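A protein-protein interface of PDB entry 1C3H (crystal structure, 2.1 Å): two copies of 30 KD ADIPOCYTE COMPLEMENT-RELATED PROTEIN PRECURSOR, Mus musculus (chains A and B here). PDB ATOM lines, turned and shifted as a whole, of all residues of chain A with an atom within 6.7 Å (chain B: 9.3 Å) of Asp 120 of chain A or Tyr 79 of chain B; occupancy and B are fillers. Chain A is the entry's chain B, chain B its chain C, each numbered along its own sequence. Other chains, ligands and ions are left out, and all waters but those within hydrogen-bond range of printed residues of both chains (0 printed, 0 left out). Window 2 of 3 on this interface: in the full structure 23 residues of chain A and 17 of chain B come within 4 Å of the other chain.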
ATOM      1  N   THR A  14     -14.035  16.610  -3.922  1.00  0.00           N
ATOM      2  CA  THR A  14     -15.318  15.907  -4.023  1.00  0.00           C
ATOM      3  C   THR A  14     -16.386  16.682  -4.793  1.00  0.00           C
ATOM      4  O   THR A  14     -16.468  17.907  -4.700  1.00  0.00           O
ATOM      5  CB  THR A  14     -15.903  15.533  -2.650  1.00  0.00           C
ATOM      6  OG1 THR A  14     -16.949  14.571  -2.832  1.00  0.00           O
ATOM      7  CG2 THR A  14     -16.465  16.763  -1.948  1.00  0.00           C
ATOM      8  N   THR A  58     -12.315   9.360  -6.756  1.00  0.00           N
ATOM      9  CA  THR A  58     -13.300   8.683  -5.939  1.00  0.00           C
ATOM     10  C   THR A  58     -14.633   8.999  -6.582  1.00  0.00           C
ATOM     11  O   THR A  58     -14.965  10.159  -6.779  1.00  0.00           O
ATOM     12  CB  THR A  58     -13.284   9.220  -4.506  1.00  0.00           C
ATOM     13  OG1 THR A  58     -11.978   9.027  -3.946  1.00  0.00           O
ATOM     14  CG2 THR A  58     -14.317   8.499  -3.652  1.00  0.00           C
ATOM     15  N   TYR A  60     -18.762   8.577  -6.437  1.00  0.00           N
ATOM     16  CA  TYR A  60     -19.899   8.265  -5.586  1.00  0.00           C
ATOM     17  C   TYR A  60     -21.106   7.802  -6.390  1.00  0.00           C
ATOM     18  O   TYR A  60     -21.943   8.601  -6.805  1.00  0.00           O
ATOM     19  CB  TYR A  60     -20.265   9.487  -4.740  1.00  0.00           C
ATOM     20  CG  TYR A  60     -19.188   9.879  -3.752  1.00  0.00           C
ATOM     21  CD1 TYR A  60     -18.967   9.127  -2.598  1.00  0.00           C
ATOM     22  CD2 TYR A  60     -18.380  10.995  -3.976  1.00  0.00           C
ATOM     23  CE1 TYR A  60     -17.967   9.476  -1.690  1.00  0.00           C
ATOM     24  CE2 TYR A  60     -17.378  11.353  -3.076  1.00  0.00           C
ATOM     25  CZ  TYR A  60     -17.178  10.587  -1.936  1.00  0.00           C
ATOM     26  OH  TYR A  60     -16.184  10.928  -1.047  1.00  0.00           O
ATOM     27  N   GLN A  89     -13.140   3.859  -5.994  1.00  0.00           N
ATOM     28  CA  GLN A  89     -11.897   4.621  -6.052  1.00  0.00           C
ATOM     29  C   GLN A  89     -11.000   4.045  -7.141  1.00  0.00           C
ATOM     30  O   GLN A  89     -10.250   3.095  -6.911  1.00  0.00           O
ATOM     31  CB  GLN A  89     -11.183   4.566  -4.703  1.00  0.00           C
ATOM     32  CG  GLN A  89     -12.102   4.847  -3.527  1.00  0.00           C
ATOM     33  CD  GLN A  89     -11.347   5.094  -2.240  1.00  0.00           C
ATOM     34  OE1 GLN A  89     -10.457   4.324  -1.870  1.00  0.00           O
ATOM     35  NE2 GLN A  89     -11.705   6.169  -1.540  1.00  0.00           N
ATOM     36  N   TYR A 118     -24.264  10.658   2.499  1.00  0.00           N
ATOM     37  CA  TYR A 118     -22.874  11.058   2.300  1.00  0.00           C
ATOM     38  C   TYR A 118     -22.021  10.921   3.561  1.00  0.00           C
ATOM     39  O   TYR A 118     -22.186   9.978   4.335  1.00  0.00           O
ATOM     40  CB  TYR A 118     -22.818  12.503   1.800  1.00  0.00           C
ATOM     41  CG  TYR A 118     -22.045  12.683   0.511  1.00  0.00           C
ATOM     42  CD1 TYR A 118     -22.504  12.132  -0.687  1.00  0.00           C
ATOM     43  CD2 TYR A 118     -20.857  13.414   0.486  1.00  0.00           C
ATOM     44  CE1 TYR A 118     -21.803  12.309  -1.877  1.00  0.00           C
ATOM     45  CE2 TYR A 118     -20.147  13.595  -0.699  1.00  0.00           C
ATOM     46  CZ  TYR A 118     -20.626  13.043  -1.875  1.00  0.00           C
ATOM     47  OH  TYR A 118     -19.937  13.242  -3.048  1.00  0.00           O
ATOM     48  N   ALA A 119     -21.105  11.867   3.751  1.00  0.00           N
ATOM     49  CA  ALA A 119     -20.213  11.876   4.907  1.00  0.00           C
ATOM     50  C   ALA A 119     -19.261  13.068   4.863  1.00  0.00           C
ATOM     51  O   ALA A 119     -19.300  13.877   3.934  1.00  0.00           O
ATOM     52  CB  ALA A 119     -19.415  10.576   4.964  1.00  0.00           C
ATOM     53  N   ASP A 120     -18.407  13.165   5.879  1.00  0.00           N
ATOM     54  CA  ASP A 120     -17.429  14.247   5.987  1.00  0.00           C
ATOM     55  C   ASP A 120     -16.770  14.534   4.641  1.00  0.00           C
ATOM     56  O   ASP A 120     -16.779  15.668   4.162  1.00  0.00           O
ATOM     57  CB  ASP A 120     -16.350  13.880   7.012  1.00  0.00           C
ATOM     58  CG  ASP A 120     -15.582  12.622   6.629  1.00  0.00           C
ATOM     59  OD1 ASP A 120     -16.200  11.537   6.556  1.00  0.00           O
ATOM     60  OD2 ASP A 120     -14.358  12.718   6.397  1.00  0.00           O
ATOM     61  N   ASN A 121     -16.194  13.494   4.047  1.00  0.00           N
ATOM     62  CA  ASN A 121     -15.527  13.581   2.753  1.00  0.00           C
ATOM     63  C   ASN A 121     -14.093  14.089   2.855  1.00  0.00           C
ATOM     64  O   ASN A 121     -13.224  13.405   3.398  1.00  0.00           O
ATOM     65  CB  ASN A 121     -16.324  14.477   1.799  1.00  0.00           C
ATOM     66  CG  ASN A 121     -16.006  14.206   0.343  1.00  0.00           C
ATOM     67  OD1 ASN A 121     -14.855  14.307  -0.090  1.00  0.00           O
ATOM     68  ND2 ASN A 121     -17.030  13.855  -0.424  1.00  0.00           N
ATOM     69  N   VAL A 122     -13.852  15.291   2.341  1.00  0.00           N
ATOM     70  CA  VAL A 122     -12.511  15.876   2.345  1.00  0.00           C
ATOM     71  C   VAL A 122     -11.540  14.827   1.806  1.00  0.00           C
ATOM     72  O   VAL A 122     -10.615  14.394   2.496  1.00  0.00           O
ATOM     73  CB  VAL A 122     -12.071  16.299   3.762  1.00  0.00           C
ATOM     74  CG1 VAL A 122     -10.704  16.971   3.703  1.00  0.00           C
ATOM     75  CG2 VAL A 122     -13.098  17.248   4.367  1.00  0.00           C
ATOM     76  N   ASN A 123     -11.782  14.410   0.567  1.00  0.00           N
ATOM     77  CA  ASN A 123     -10.949  13.408  -0.087  1.00  0.00           C
ATOM     78  C   ASN A 123     -10.567  13.861  -1.490  1.00  0.00           C
ATOM     79  O   ASN A 123     -11.403  13.910  -2.388  1.00  0.00           O
ATOM     80  CB  ASN A 123     -11.692  12.070  -0.150  1.00  0.00           C
ATOM     81  CG  ASN A 123     -10.903  11.000  -0.875  1.00  0.00           C
ATOM     82  OD1 ASN A 123     -10.808  11.007  -2.101  1.00  0.00           O
ATOM     83  ND2 ASN A 123     -10.320  10.081  -0.120  1.00  0.00           N
ATOM     84  N   ASP A 124      -9.292  14.186  -1.667  1.00  0.00           N
ATOM     85  CA  ASP A 124      -8.796  14.651  -2.950  1.00  0.00           C
ATOM     86  C   ASP A 124      -8.762  13.613  -4.067  1.00  0.00           C
ATOM     87  O   ASP A 124      -8.213  12.525  -3.902  1.00  0.00           O
ATOM     88  CB  ASP A 124      -7.392  15.247  -2.795  1.00  0.00           C
ATOM     89  CG  ASP A 124      -7.411  16.639  -2.194  1.00  0.00           C
ATOM     90  OD1 ASP A 124      -8.169  17.492  -2.705  1.00  0.00           O
ATOM     91  OD2 ASP A 124      -6.666  16.887  -1.221  1.00  0.00           O
ATOM     92  N   TYR B  55       2.799   7.933  -4.482  1.00  0.00           N
ATOM     93  CA  TYR B  55       2.954   7.067  -3.328  1.00  0.00           C
ATOM     94  C   TYR B  55       1.884   5.988  -3.326  1.00  0.00           C
ATOM     95  O   TYR B  55       0.799   6.169  -3.872  1.00  0.00           O
ATOM     96  CB  TYR B  55       2.874   7.880  -2.030  1.00  0.00           C
ATOM     97  CG  TYR B  55       1.536   8.539  -1.806  1.00  0.00           C
ATOM     98  CD1 TYR B  55       0.473   7.835  -1.250  1.00  0.00           C
ATOM     99  CD2 TYR B  55       1.330   9.871  -2.158  1.00  0.00           C
ATOM    100  CE1 TYR B  55      -0.758   8.440  -1.049  1.00  0.00           C
ATOM    101  CE2 TYR B  55       0.105  10.483  -1.961  1.00  0.00           C
ATOM    102  CZ  TYR B  55      -0.933   9.763  -1.408  1.00  0.00           C
ATOM    103  OH  TYR B  55      -2.158  10.370  -1.228  1.00  0.00           O
ATOM    104  N   LYS B  62      -7.315   1.875  12.081  1.00  0.00           N
ATOM    105  CA  LYS B  62      -8.693   2.198  11.722  1.00  0.00           C
ATOM    106  C   LYS B  62      -8.894   3.644  11.279  1.00  0.00           C
ATOM    107  O   LYS B  62      -8.110   4.526  11.629  1.00  0.00           O
ATOM    108  CB  LYS B  62      -9.619   1.879  12.899  1.00  0.00           C
ATOM    109  N   ASP B  63      -9.958   3.869  10.511  1.00  0.00           N
ATOM    110  CA  ASP B  63     -10.311   5.195   9.998  1.00  0.00           C
ATOM    111  C   ASP B  63      -9.064   5.990   9.618  1.00  0.00           C
ATOM    112  O   ASP B  63      -8.780   7.042  10.196  1.00  0.00           O
ATOM    113  CB  ASP B  63     -11.111   5.973  11.042  1.00  0.00           C
ATOM    114  CG  ASP B  63     -11.853   7.152  10.444  1.00  0.00           C
ATOM    115  OD1 ASP B  63     -12.140   8.116  11.184  1.00  0.00           O
ATOM    116  OD2 ASP B  63     -12.163   7.110   9.231  1.00  0.00           O
ATOM    117  N   VAL B  64      -8.333   5.483   8.633  1.00  0.00           N
ATOM    118  CA  VAL B  64      -7.104   6.114   8.183  1.00  0.00           C
ATOM    119  C   VAL B  64      -7.300   7.275   7.216  1.00  0.00           C
ATOM    120  O   VAL B  64      -8.153   7.237   6.330  1.00  0.00           O
ATOM    121  CB  VAL B  64      -6.179   5.079   7.510  1.00  0.00           C
ATOM    122  CG1 VAL B  64      -4.854   5.730   7.119  1.00  0.00           C
ATOM    123  CG2 VAL B  64      -5.951   3.909   8.446  1.00  0.00           C
ATOM    124  N   LYS B  65      -6.492   8.311   7.410  1.00  0.00           N
ATOM    125  CA  LYS B  65      -6.509   9.492   6.559  1.00  0.00           C
ATOM    126  C   LYS B  65      -5.046   9.730   6.209  1.00  0.00           C
ATOM    127  O   LYS B  65      -4.180   9.720   7.085  1.00  0.00           O
ATOM    128  CB  LYS B  65      -7.079  10.690   7.312  1.00  0.00           C
ATOM    129  CG  LYS B  65      -8.471  10.436   7.860  1.00  0.00           C
ATOM    130  CD  LYS B  65      -8.884  11.479   8.881  1.00  0.00           C
ATOM    131  CE  LYS B  65     -10.148  11.034   9.589  1.00  0.00           C
ATOM    132  NZ  LYS B  65      -9.966   9.671  10.169  1.00  0.00           N
ATOM    133  N   VAL B  66      -4.770   9.910   4.925  1.00  0.00           N
ATOM    134  CA  VAL B  66      -3.404  10.126   4.483  1.00  0.00           C
ATOM    135  C   VAL B  66      -3.220  11.546   3.985  1.00  0.00           C
ATOM    136  O   VAL B  66      -4.059  12.075   3.261  1.00  0.00           O
ATOM    137  CB  VAL B  66      -3.018   9.148   3.348  1.00  0.00           C
ATOM    138  CG1 VAL B  66      -1.546   9.316   2.992  1.00  0.00           C
ATOM    139  CG2 VAL B  66      -3.296   7.724   3.779  1.00  0.00           C
ATOM    140  N   SER B  67      -2.120  12.161   4.389  1.00  0.00           N
ATOM    141  CA  SER B  67      -1.828  13.516   3.964  1.00  0.00           C
ATOM    142  C   SER B  67      -0.432  13.615   3.384  1.00  0.00           C
ATOM    143  O   SER B  67       0.530  13.098   3.952  1.00  0.00           O
ATOM    144  CB  SER B  67      -1.945  14.501   5.137  1.00  0.00           C
ATOM    145  OG  SER B  67      -3.276  14.600   5.611  1.00  0.00           O
ATOM    146  N   LEU B  76      -2.234  17.528  -0.174  1.00  0.00           N
ATOM    147  CA  LEU B  76      -3.044  16.440  -0.708  1.00  0.00           C
ATOM    148  C   LEU B  76      -3.626  15.664   0.478  1.00  0.00           C
ATOM    149  O   LEU B  76      -2.914  15.335   1.422  1.00  0.00           O
ATOM    150  CB  LEU B  76      -2.168  15.532  -1.579  1.00  0.00           C
ATOM    151  CG  LEU B  76      -2.814  14.530  -2.541  1.00  0.00           C
ATOM    152  CD1 LEU B  76      -3.596  13.487  -1.764  1.00  0.00           C
ATOM    153  CD2 LEU B  76      -3.717  15.276  -3.510  1.00  0.00           C
ATOM    154  N   PHE B  77      -4.920  15.374   0.432  1.00  0.00           N
ATOM    155  CA  PHE B  77      -5.561  14.663   1.532  1.00  0.00           C
ATOM    156  C   PHE B  77      -6.371  13.471   1.037  1.00  0.00           C
ATOM    157  O   PHE B  77      -7.334  13.632   0.289  1.00  0.00           O
ATOM    158  CB  PHE B  77      -6.459  15.629   2.315  1.00  0.00           C
ATOM    159  CG  PHE B  77      -6.810  15.150   3.695  1.00  0.00           C
ATOM    160  CD1 PHE B  77      -7.824  14.218   3.892  1.00  0.00           C
ATOM    161  CD2 PHE B  77      -6.112  15.621   4.803  1.00  0.00           C
ATOM    162  CE1 PHE B  77      -8.137  13.760   5.177  1.00  0.00           C
ATOM    163  CE2 PHE B  77      -6.416  15.171   6.088  1.00  0.00           C
ATOM    164  CZ  PHE B  77      -7.430  14.240   6.276  1.00  0.00           C
ATOM    165  N   THR B  78      -5.969  12.279   1.464  1.00  0.00           N
ATOM    166  CA  THR B  78      -6.641  11.046   1.066  1.00  0.00           C
ATOM    167  C   THR B  78      -7.409  10.408   2.218  1.00  0.00           C
ATOM    168  O   THR B  78      -6.881  10.221   3.311  1.00  0.00           O
ATOM    169  CB  THR B  78      -5.629  10.006   0.519  1.00  0.00           C
ATOM    170  OG1 THR B  78      -5.011  10.511  -0.671  1.00  0.00           O
ATOM    171  CG2 THR B  78      -6.329   8.695   0.198  1.00  0.00           C
ATOM    172  N   TYR B  79      -8.665  10.073   1.959  1.00  0.00           N
ATOM    173  CA  TYR B  79      -9.516   9.439   2.954  1.00  0.00           C
ATOM    174  C   TYR B  79     -10.340   8.363   2.259  1.00  0.00           C
ATOM    175  O   TYR B  79     -11.516   8.566   1.960  1.00  0.00           O
ATOM    176  CB  TYR B  79     -10.446  10.469   3.598  1.00  0.00           C
ATOM    177  CG  TYR B  79     -11.354   9.883   4.655  1.00  0.00           C
ATOM    178  CD1 TYR B  79     -10.832   9.345   5.829  1.00  0.00           C
ATOM    179  CD2 TYR B  79     -12.738   9.854   4.475  1.00  0.00           C
ATOM    180  CE1 TYR B  79     -11.661   8.791   6.800  1.00  0.00           C
ATOM    181  CE2 TYR B  79     -13.581   9.300   5.442  1.00  0.00           C
ATOM    182  CZ  TYR B  79     -13.034   8.769   6.602  1.00  0.00           C
ATOM    183  OH  TYR B  79     -13.856   8.209   7.555  1.00  0.00           O
ATOM    184  N   ASP B  80      -9.709   7.226   1.988  1.00  0.00           N
ATOM    185  CA  ASP B  80     -10.382   6.121   1.319  1.00  0.00           C
ATOM    186  C   ASP B  80     -11.650   5.730   2.067  1.00  0.00           C
ATOM    187  O   ASP B  80     -11.590   5.232   3.190  1.00  0.00           O
ATOM    188  CB  ASP B  80      -9.441   4.916   1.214  1.00  0.00           C
ATOM    189  CG  ASP B  80      -8.218   5.203   0.358  1.00  0.00           C
ATOM    190  OD1 ASP B  80      -8.388   5.605  -0.810  1.00  0.00           O
ATOM    191  OD2 ASP B  80      -7.086   5.023   0.855  1.00  0.00           O
ATOM    192  N   GLN B  81     -12.797   5.965   1.436  1.00  0.00           N
ATOM    193  CA  GLN B  81     -14.088   5.650   2.039  1.00  0.00           C
ATOM    194  C   GLN B  81     -14.377   4.154   2.018  1.00  0.00           C
ATOM    195  O   GLN B  81     -15.316   3.688   2.662  1.00  0.00           O
ATOM    196  CB  GLN B  81     -15.194   6.405   1.314  1.00  0.00           C
ATOM    197  N   TYR B  82     -13.565   3.405   1.278  1.00  0.00           N
ATOM    198  CA  TYR B  82     -13.740   1.962   1.175  1.00  0.00           C
ATOM    199  C   TYR B  82     -12.748   1.215   2.061  1.00  0.00           C
ATOM    200  O   TYR B  82     -12.046   0.313   1.598  1.00  0.00           O
ATOM    201  CB  TYR B  82     -13.578   1.522  -0.278  1.00  0.00           C
ATOM    202  N   GLN B  83     -12.697   1.592   3.337  1.00  0.00           N
ATOM    203  CA  GLN B  83     -11.791   0.955   4.287  1.00  0.00           C
ATOM    204  C   GLN B  83     -12.432  -0.216   5.022  1.00  0.00           C
ATOM    205  O   GLN B  83     -13.422  -0.050   5.738  1.00  0.00           O
ATOM    206  CB  GLN B  83     -11.282   1.972   5.313  1.00  0.00           C
ATOM    207  CG  GLN B  83     -10.284   2.975   4.763  1.00  0.00           C
ATOM    208  CD  GLN B  83      -9.694   3.859   5.845  1.00  0.00           C
ATOM    209  OE1 GLN B  83      -9.112   3.369   6.815  1.00  0.00           O
ATOM    210  NE2 GLN B  83      -9.837   5.169   5.683  1.00  0.00           N
ATOM    211  N   ASP B  88      -5.629  -0.033   5.603  1.00  0.00           N
ATOM    212  CA  ASP B  88      -5.985   0.892   4.535  1.00  0.00           C
ATOM    213  C   ASP B  88      -4.849   1.011   3.528  1.00  0.00           C
ATOM    214  O   ASP B  88      -3.686   1.146   3.901  1.00  0.00           O
ATOM    215  CB  ASP B  88      -6.312   2.272   5.111  1.00  0.00           C
ATOM    216  CG  ASP B  88      -6.661   3.282   4.036  1.00  0.00           C
ATOM    217  OD1 ASP B  88      -7.571   3.000   3.229  1.00  0.00           O
ATOM    218  OD2 ASP B  88      -6.030   4.359   3.997  1.00  0.00           O
ATOM    219  N   GLN B  89      -5.194   0.952   2.247  1.00  0.00           N
ATOM    220  CA  GLN B  89      -4.203   1.053   1.186  1.00  0.00           C
ATOM    221  C   GLN B  89      -4.469   2.289   0.332  1.00  0.00           C
ATOM    222  O   GLN B  89      -5.335   2.279  -0.547  1.00  0.00           O
ATOM    223  CB  GLN B  89      -4.236  -0.208   0.324  1.00  0.00           C
ATOM    224  CG  GLN B  89      -3.181  -0.241  -0.762  1.00  0.00           C
ATOM    225  CD  GLN B  89      -2.968  -1.638  -1.308  1.00  0.00           C
ATOM    226  OE1 GLN B  89      -3.925  -2.338  -1.648  1.00  0.00           O
ATOM    227  NE2 GLN B  89      -1.707  -2.051  -1.402  1.00  0.00           N
ATOM    228  N   ALA B  90      -3.719   3.352   0.595  1.00  0.00           N
ATOM    229  CA  ALA B  90      -3.889   4.603  -0.134  1.00  0.00           C
ATOM    230  C   ALA B  90      -2.786   4.880  -1.150  1.00  0.00           C
ATOM    231  O   ALA B  90      -1.636   4.477  -0.977  1.00  0.00           O
ATOM    232  CB  ALA B  90      -3.977   5.758   0.848  1.00  0.00           C
ATOM    233  N   SER B  91      -3.151   5.577  -2.216  1.00  0.00           N
ATOM    234  CA  SER B  91      -2.190   5.933  -3.245  1.00  0.00           C
ATOM    235  C   SER B  91      -2.570   7.294  -3.799  1.00  0.00           C
ATOM    236  O   SER B  91      -3.712   7.725  -3.676  1.00  0.00           O
ATOM    237  CB  SER B  91      -2.181   4.891  -4.373  1.00  0.00           C
ATOM    238  OG  SER B  91      -3.391   4.920  -5.107  1.00  0.00           O
ATOM    239  N   TYR B 109      -3.135   9.450   9.683  1.00  0.00           N
ATOM    240  CA  TYR B 109      -3.960   9.735  10.845  1.00  0.00           C
ATOM    241  C   TYR B 109      -4.959   8.597  10.983  1.00  0.00           C
ATOM    242  O   TYR B 109      -5.482   8.102   9.982  1.00  0.00           O
ATOM    243  CB  TYR B 109      -4.695  11.061  10.650  1.00  0.00           C
ATOM    244  CG  TYR B 109      -3.759  12.209  10.376  1.00  0.00           C
ATOM    245  CD1 TYR B 109      -2.920  12.698  11.376  1.00  0.00           C
ATOM    246  CD2 TYR B 109      -3.662  12.767   9.100  1.00  0.00           C
ATOM    247  CE1 TYR B 109      -2.002  13.710  11.115  1.00  0.00           C
ATOM    248  CE2 TYR B 109      -2.746  13.780   8.828  1.00  0.00           C
ATOM    249  CZ  TYR B 109      -1.918  14.245   9.841  1.00  0.00           C
ATOM    250  OH  TYR B 109      -1.002  15.237   9.580  1.00  0.00           O
ATOM    251  N   GLY B 110      -5.214   8.180  12.219  1.00  0.00           N
ATOM    252  CA  GLY B 110      -6.153   7.097  12.457  1.00  0.00           C
ATOM    253  C   GLY B 110      -5.987   6.469  13.828  1.00  0.00           C
ATOM    254  O   GLY B 110      -5.178   6.925  14.634  1.00  0.00           O
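The side-chain amide nitrogen (NE2) of Gln 89 of chain A sits close to the backbone NH (N) of Gln 81 of chain B (3.2 Å). OE1 of Gln 89 of chain A sits close to OD1 of Asp 80 of chain B (2.7 Å). N of Asp 124 of chain A sits at hydrogen-bond distance from O of Phe 77 of chain B (2.8 Å). The side-chain amide nitrogen of Asn 123 of chain A sits close to the backbone NH of Tyr 79 of chain B (2.7 Å).
The side-chain hydroxyl (OH) of Tyr 55 of chain B sits at hydrogen-bond distance from the side-chain hydroxyl (OG1) of Thr 78 of chain B (2.9 Å). OD2 of Asp 63 of chain B sits at hydrogen-bond distance from OH of Tyr 79 of chain B. The side-chain hydroxyl of Thr 14 of chain A sits at hydrogen-bond distance from the side-chain amide nitrogen of Asn 121 of chain A (2.5 Å). OH of Tyr 60 of chain A lies within hydrogen-bond range of ND2 of Asn 121 of chain A (3.1 Å). The backbone NH (N) of Thr 78 of chain B sits at hydrogen-bond distance from the backbone carbonyl oxygen (O) of Val 66 of chain B (2.6 Å). The side-chain amide nitrogen of Gln 83 of chain B sits close to the backbone carbonyl oxygen of Asp 80 of chain B (3.0 Å).
CE2 of Tyr 79 of chain B touches OD1 of Asp 120 of chain A, at 3.6 Å. Asn 121 of chain A touches Tyr 79 of chain B. O of Val 122 of chain A touches CD1 of Phe 77 of chain B, at 3.1 Å. O of Phe 77 of chain B touches CA of Asn 123 of chain A, 3.6 Å away. ND2 of Asn 123 of chain A touches C of Thr 78 of chain B (3.7 Å). N of Asp 80 of chain B touches ND2 of Asn 123 of chain A (3.6 Å). CA of Leu 76 of chain B touches OD2 of Asp 124 of chain A, at 3.7 Å.
No residue of chain B comes within 4 Å of Ala 119 of chain A. Asp 120 of chain A touches one residue of chain B. Asn 121 of chain A touches just one residue of chain B: Tyr 79. Of the printed residues of chain B, Val 122 of chain A touches Phe 77 (3.1 Å). Of the printed residues of chain A, Leu 76 of chain B touches Asp 124 (3.7 Å). Of the printed residues of chain A, Phe 77 of chain B touches Val 122, Asn 123 and Asp 124. Of the printed residues of chain A, Thr 78 of chain B touches Asn 123 (3.7 Å). Of chain A, only Asp 120 (3.6 Å), Asn 121 (3.7 Å) and Asn 123 (2.7 Å) come within 4 Å of Tyr 79 of chain B. Ser 91 of chain B touches none of the printed residues of chain A. The nearest residue of chain A that does not touch Tyr 79 of chain B is Val 122 of chain A (4.1 Å). The nearest printed residue of chain B that does not touch Asn 123 of chain A is Gln 81 of chain B (5.0 Å).
Printed residues of chain A that touch a printed residue of chain B: Gln 89, Asp 120, Asn 121, Val 122, Asn 123 and Asp 124. Hydrophobic or aromatic side chains of chain A within 4 Å of the printed part of chain B: Val 122. Along chain A the printed residues that touch a printed residue of chain B span positions 89 to 124. Of the 21 printed residues of chain B, 6 touch a printed residue of chain A. Printed residues of chain B that touch a printed residue of chain A: Leu 76, Phe 77, Thr 78, Tyr 79, Asp 80 and Gln 81. Along chain B the printed residues that touch a printed residue of chain A span positions 76 to 81. Among the printed residues, no Asp or Glu carboxylate lies within 4 Å of a Lys or Arg side-chain nitrogen of the other chain.
Position printed for both chains: 89.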
